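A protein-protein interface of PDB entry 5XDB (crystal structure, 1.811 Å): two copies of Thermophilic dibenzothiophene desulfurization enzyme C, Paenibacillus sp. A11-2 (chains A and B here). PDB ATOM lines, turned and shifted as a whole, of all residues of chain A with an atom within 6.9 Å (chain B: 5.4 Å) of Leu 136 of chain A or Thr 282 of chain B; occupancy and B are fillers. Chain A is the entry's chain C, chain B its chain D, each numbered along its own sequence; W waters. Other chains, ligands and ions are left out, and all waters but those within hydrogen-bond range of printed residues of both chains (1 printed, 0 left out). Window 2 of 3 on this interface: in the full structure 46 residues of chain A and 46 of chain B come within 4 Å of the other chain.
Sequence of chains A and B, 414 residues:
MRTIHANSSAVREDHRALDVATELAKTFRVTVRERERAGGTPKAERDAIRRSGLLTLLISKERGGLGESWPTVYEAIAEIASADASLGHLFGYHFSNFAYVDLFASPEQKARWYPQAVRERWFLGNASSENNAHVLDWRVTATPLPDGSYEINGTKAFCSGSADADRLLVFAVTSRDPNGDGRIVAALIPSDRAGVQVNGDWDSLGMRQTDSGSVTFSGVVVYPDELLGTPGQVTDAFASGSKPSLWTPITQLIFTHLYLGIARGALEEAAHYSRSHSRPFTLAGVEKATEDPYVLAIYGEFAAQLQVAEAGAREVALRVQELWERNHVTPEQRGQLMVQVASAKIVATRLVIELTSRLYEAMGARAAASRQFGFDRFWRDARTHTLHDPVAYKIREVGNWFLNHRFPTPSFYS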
ATOM      1  N   ASN A 132      15.558 -18.428 -17.373  1.00  0.00           N
ATOM      2  CA  ASN A 132      15.031 -17.101 -17.114  1.00  0.00           C
ATOM      3  C   ASN A 132      16.023 -16.319 -16.244  1.00  0.00           C
ATOM      4  O   ASN A 132      17.219 -16.627 -16.227  1.00  0.00           O
ATOM      5  CB  ASN A 132      13.633 -17.244 -16.507  1.00  0.00           C
ATOM      6  CG  ASN A 132      12.664 -17.917 -17.467  1.00  0.00           C
ATOM      7  OD1 ASN A 132      12.604 -17.558 -18.647  1.00  0.00           O
ATOM      8  ND2 ASN A 132      11.930 -18.914 -16.980  1.00  0.00           N
ATOM      9  N   ALA A 133      15.533 -15.302 -15.523  1.00  0.00           N
ATOM     10  CA  ALA A 133      16.424 -14.372 -14.828  1.00  0.00           C
ATOM     11  C   ALA A 133      17.195 -15.039 -13.696  1.00  0.00           C
ATOM     12  O   ALA A 133      18.303 -14.602 -13.366  1.00  0.00           O
ATOM     13  CB  ALA A 133      15.627 -13.188 -14.285  1.00  0.00           C
ATOM     14  N   HIS A 134      16.628 -16.074 -13.084  1.00  0.00           N
ATOM     15  CA  HIS A 134      17.304 -16.844 -12.045  1.00  0.00           C
ATOM     16  C   HIS A 134      16.630 -18.206 -11.970  1.00  0.00           C
ATOM     17  O   HIS A 134      15.607 -18.446 -12.613  1.00  0.00           O
ATOM     18  CB  HIS A 134      17.268 -16.118 -10.696  1.00  0.00           C
ATOM     19  CG  HIS A 134      15.899 -15.656 -10.299  1.00  0.00           C
ATOM     20  ND1 HIS A 134      14.991 -16.476  -9.663  1.00  0.00           N
ATOM     21  CD2 HIS A 134      15.278 -14.465 -10.462  1.00  0.00           C
ATOM     22  CE1 HIS A 134      13.872 -15.807  -9.445  1.00  0.00           C
ATOM     23  NE2 HIS A 134      14.024 -14.581  -9.912  1.00  0.00           N
ATOM     24  N   VAL A 135      17.210 -19.100 -11.163  1.00  0.00           N
ATOM     25  CA  VAL A 135      16.750 -20.486 -11.143  1.00  0.00           C
ATOM     26  C   VAL A 135      15.400 -20.678 -10.464  1.00  0.00           C
ATOM     27  O   VAL A 135      14.846 -21.779 -10.523  1.00  0.00           O
ATOM     28  CB  VAL A 135      17.802 -21.399 -10.478  1.00  0.00           C
ATOM     29  CG1 VAL A 135      19.061 -21.465 -11.348  1.00  0.00           C
ATOM     30  CG2 VAL A 135      18.130 -20.909  -9.070  1.00  0.00           C
ATOM     31  N   LEU A 136      14.854 -19.654  -9.816  1.00  0.00           N
ATOM     32  CA  LEU A 136      13.500 -19.750  -9.283  1.00  0.00           C
ATOM     33  C   LEU A 136      12.445 -19.214 -10.245  1.00  0.00           C
ATOM     34  O   LEU A 136      11.246 -19.401 -10.003  1.00  0.00           O
ATOM     35  CB  LEU A 136      13.411 -19.009  -7.947  1.00  0.00           C
ATOM     36  CG  LEU A 136      14.378 -19.618  -6.929  1.00  0.00           C
ATOM     37  CD1 LEU A 136      14.216 -19.023  -5.535  1.00  0.00           C
ATOM     38  CD2 LEU A 136      14.196 -21.129  -6.912  1.00  0.00           C
ATOM     39  N   ASP A 137      12.863 -18.577 -11.334  1.00  0.00           N
ATOM     40  CA  ASP A 137      11.962 -17.905 -12.268  1.00  0.00           C
ATOM     41  C   ASP A 137      11.476 -18.939 -13.282  1.00  0.00           C
ATOM     42  O   ASP A 137      12.103 -19.172 -14.317  1.00  0.00           O
ATOM     43  CB  ASP A 137      12.693 -16.735 -12.918  1.00  0.00           C
ATOM     44  CG  ASP A 137      11.819 -15.928 -13.854  1.00  0.00           C
ATOM     45  OD1 ASP A 137      10.604 -16.208 -13.953  1.00  0.00           O
ATOM     46  OD2 ASP A 137      12.365 -14.997 -14.493  1.00  0.00           O
ATOM     47  N   TRP A 138      10.350 -19.585 -12.972  1.00  0.00           N
ATOM     48  CA  TRP A 138       9.745 -20.568 -13.860  1.00  0.00           C
ATOM     49  C   TRP A 138       8.604 -19.933 -14.646  1.00  0.00           C
ATOM     50  O   TRP A 138       7.847 -19.111 -14.117  1.00  0.00           O
ATOM     51  CB  TRP A 138       9.226 -21.787 -13.091  1.00  0.00           C
ATOM     52  CG  TRP A 138      10.288 -22.804 -12.798  1.00  0.00           C
ATOM     53  CD1 TRP A 138      11.640 -22.646 -12.952  1.00  0.00           C
ATOM     54  CD2 TRP A 138      10.093 -24.135 -12.311  1.00  0.00           C
ATOM     55  NE1 TRP A 138      12.296 -23.801 -12.585  1.00  0.00           N
ATOM     56  CE2 TRP A 138      11.369 -24.728 -12.187  1.00  0.00           C
ATOM     57  CE3 TRP A 138       8.966 -24.886 -11.962  1.00  0.00           C
ATOM     58  CZ2 TRP A 138      11.546 -26.033 -11.727  1.00  0.00           C
ATOM     59  CZ3 TRP A 138       9.146 -26.181 -11.508  1.00  0.00           C
ATOM     60  CH2 TRP A 138      10.422 -26.740 -11.394  1.00  0.00           C
ATOM     61  N   ARG A 139       8.499 -20.313 -15.917  1.00  0.00           N
ATOM     62  CA  ARG A 139       7.477 -19.759 -16.786  1.00  0.00           C
ATOM     63  C   ARG A 139       6.795 -20.792 -17.667  1.00  0.00           C
ATOM     64  O   ARG A 139       5.821 -20.442 -18.338  1.00  0.00           O
ATOM     65  CB  ARG A 139       8.075 -18.656 -17.666  1.00  0.00           C
ATOM     66  CG  ARG A 139       8.715 -17.543 -16.850  1.00  0.00           C
ATOM     67  CD  ARG A 139       9.221 -16.437 -17.752  1.00  0.00           C
ATOM     68  NE  ARG A 139      10.110 -15.525 -17.042  1.00  0.00           N
ATOM     69  CZ  ARG A 139      10.698 -14.474 -17.601  1.00  0.00           C
ATOM     70  NH1 ARG A 139      10.490 -14.189 -18.884  1.00  0.00           N
ATOM     71  NH2 ARG A 139      11.493 -13.702 -16.872  1.00  0.00           N
ATOM     72  N   TYR A 413      17.612 -27.965  -4.748  1.00  0.00           N
ATOM     73  CA  TYR A 413      19.066 -27.906  -4.673  1.00  0.00           C
ATOM     74  C   TYR A 413      19.626 -28.252  -3.298  1.00  0.00           C
ATOM     75  O   TYR A 413      20.825 -28.525  -3.187  1.00  0.00           O
ATOM     76  CB  TYR A 413      19.566 -26.508  -5.073  1.00  0.00           C
ATOM     77  CG  TYR A 413      19.149 -26.086  -6.466  1.00  0.00           C
ATOM     78  CD1 TYR A 413      19.913 -26.427  -7.577  1.00  0.00           C
ATOM     79  CD2 TYR A 413      17.980 -25.363  -6.668  1.00  0.00           C
ATOM     80  CE1 TYR A 413      19.523 -26.049  -8.863  1.00  0.00           C
ATOM     81  CE2 TYR A 413      17.582 -24.978  -7.941  1.00  0.00           C
ATOM     82  CZ  TYR A 413      18.357 -25.320  -9.032  1.00  0.00           C
ATOM     83  OH  TYR A 413      17.964 -24.941 -10.299  1.00  0.00           O
ATOM     84  N   PRO B 280      21.798 -14.252 -10.437  1.00  0.00           N
ATOM     85  CA  PRO B 280      21.957 -14.312  -8.980  1.00  0.00           C
ATOM     86  C   PRO B 280      21.406 -15.617  -8.434  1.00  0.00           C
ATOM     87  O   PRO B 280      20.427 -16.167  -8.948  1.00  0.00           O
ATOM     88  CB  PRO B 280      21.146 -13.110  -8.483  1.00  0.00           C
ATOM     89  CG  PRO B 280      20.077 -12.937  -9.533  1.00  0.00           C
ATOM     90  CD  PRO B 280      20.715 -13.333 -10.843  1.00  0.00           C
ATOM     91  N   PHE B 281      22.052 -16.127  -7.383  1.00  0.00           N
ATOM     92  CA  PHE B 281      21.578 -17.355  -6.745  1.00  0.00           C
ATOM     93  C   PHE B 281      20.476 -16.964  -5.765  1.00  0.00           C
ATOM     94  O   PHE B 281      20.712 -16.737  -4.574  1.00  0.00           O
ATOM     95  CB  PHE B 281      22.718 -18.110  -6.064  1.00  0.00           C
ATOM     96  CG  PHE B 281      22.377 -19.541  -5.730  1.00  0.00           C
ATOM     97  CD1 PHE B 281      22.044 -20.440  -6.738  1.00  0.00           C
ATOM     98  CD2 PHE B 281      22.388 -19.990  -4.416  1.00  0.00           C
ATOM     99  CE1 PHE B 281      21.715 -21.759  -6.441  1.00  0.00           C
ATOM    100  CE2 PHE B 281      22.067 -21.308  -4.109  1.00  0.00           C
ATOM    101  CZ  PHE B 281      21.731 -22.198  -5.127  1.00  0.00           C
ATOM    102  N   THR B 282      19.250 -16.867  -6.285  1.00  0.00           N
ATOM    103  CA  THR B 282      18.130 -16.390  -5.480  1.00  0.00           C
ATOM    104  C   THR B 282      17.741 -17.366  -4.385  1.00  0.00           C
ATOM    105  O   THR B 282      17.150 -16.940  -3.386  1.00  0.00           O
ATOM    106  CB  THR B 282      16.922 -16.116  -6.371  1.00  0.00           C
ATOM    107  OG1 THR B 282      16.777 -17.201  -7.299  1.00  0.00           O
ATOM    108  CG2 THR B 282      17.115 -14.805  -7.123  1.00  0.00           C
ATOM    109  N   LEU B 283      18.045 -18.659  -4.552  1.00  0.00           N
ATOM    110  CA  LEU B 283      17.821 -19.616  -3.472  1.00  0.00           C
ATOM    111  C   LEU B 283      18.427 -19.128  -2.165  1.00  0.00           C
ATOM    112  O   LEU B 283      17.946 -19.491  -1.087  1.00  0.00           O
ATOM    113  CB  LEU B 283      18.420 -20.982  -3.824  1.00  0.00           C
ATOM    114  CG  LEU B 283      17.618 -22.043  -4.585  1.00  0.00           C
ATOM    115  CD1 LEU B 283      16.345 -22.429  -3.837  1.00  0.00           C
ATOM    116  CD2 LEU B 283      17.303 -21.580  -6.001  1.00  0.00           C
ATOM    117  N   ALA B 284      19.489 -18.324  -2.237  1.00  0.00           N
ATOM    118  CA  ALA B 284      20.167 -17.829  -1.045  1.00  0.00           C
ATOM    119  C   ALA B 284      19.922 -16.348  -0.801  1.00  0.00           C
ATOM    120  O   ALA B 284      20.619 -15.744   0.018  1.00  0.00           O
ATOM    121  CB  ALA B 284      21.673 -18.097  -1.134  1.00  0.00           C
ATOM    122  N   GLY B 285      18.957 -15.746  -1.495  1.00  0.00           N
ATOM    123  CA  GLY B 285      18.624 -14.352  -1.266  1.00  0.00           C
ATOM    124  C   GLY B 285      19.494 -13.344  -1.978  1.00  0.00           C
ATOM    125  O   GLY B 285      19.375 -12.146  -1.708  1.00  0.00           O
ATOM    126  N   VAL B 286      20.365 -13.785  -2.883  1.00  0.00           N
ATOM    127  CA  VAL B 286      21.180 -12.857  -3.658  1.00  0.00           C
ATOM    128  C   VAL B 286      20.322 -12.198  -4.729  1.00  0.00           C
ATOM    129  O   VAL B 286      19.512 -12.860  -5.395  1.00  0.00           O
ATOM    130  CB  VAL B 286      22.376 -13.595  -4.289  1.00  0.00           C
ATOM    131  CG1 VAL B 286      23.201 -12.654  -5.150  1.00  0.00           C
ATOM    132  CG2 VAL B 286      23.252 -14.246  -3.203  1.00  0.00           C
HETATM  133  O   HOH W   1      19.835 -18.066 -10.602  1.00  0.00           O
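Water W1 lies within hydrogen-bond range of the backbone carbonyl oxygen (O) of Pro 280 of chain B (2.6 Å) and the backbone NH (N) of Val 135 of chain A (2.9 Å).
Printed residues of chain A that touch a printed residue of chain B: Ala 133, His 134, Val 135, Leu 136 and Tyr 413. Of the 7 printed residues of chain B, 3 touch a printed residue of chain A. Hydrophobic or aromatic side chains of chain B within 4 Å of the printed part of chain A: Pro 280 and Leu 283. Among the printed residues, no Asp or Glu carboxylate lies within 4 Å of a Lys or Arg side-chain nitrogen of the other chain.
No position is printed for both chains.
Ala 133 of chain A touches Pro 280 of chain B. O of Pro 280 of chain B touches CB of His 134 of chain A, at 3.6 Å. CG2 of Val 135 of chain A touches CD2 of Leu 283 of chain B, at 3.2 Å. Leu 136 of chain A touches Thr 282 of chain B (CG to OG1, 3.4 Å). Leu 136 of chain A touches Leu 283 of chain B. Tyr 413 of chain A touches Leu 283 of chain B (CD2 to CD2, 3.9 Å).
Leu 136 of chain A touches just these residues of chain B: Thr 282 and Leu 283. Of chain A, only His 134 and Leu 136 come within 4 Å of Thr 282 of chain B. Printed residues of chain A within 4 Å of Leu 283 of chain B: Val 135, Leu 136 and Tyr 413. Of the printed residues of chain B, Ala 133 of chain A touches Pro 280 (3.7 Å). Of the printed residues of chain B, His 134 of chain A touches Pro 280 and Thr 282. The nearest printed residue of chain B that does not touch Leu 136 of chain A is Ala 284 of chain B (6.3 Å). The nearest residue of chain A that does not touch Thr 282 of chain B is Val 135 of chain A (4.3 Å).
The backbone NH (N) of Ala 133 of chain A sits at hydrogen-bond distance from the side-chain carboxylate (OD2) of Asp 137 of chain A (3.3 Å). ND1 of His 134 of chain A lies close to N of Leu 136 of chain A. ND1 of His 134 of chain A is in hydrogen-bond range of N of Asp 137 of chain A, 3.4 Å away.
A ring nitrogen (ND1) of His 134 of chain A is in hydrogen-bond range of the side-chain hydroxyl (OG1) of Thr 282 of chain B (3.1 Å).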
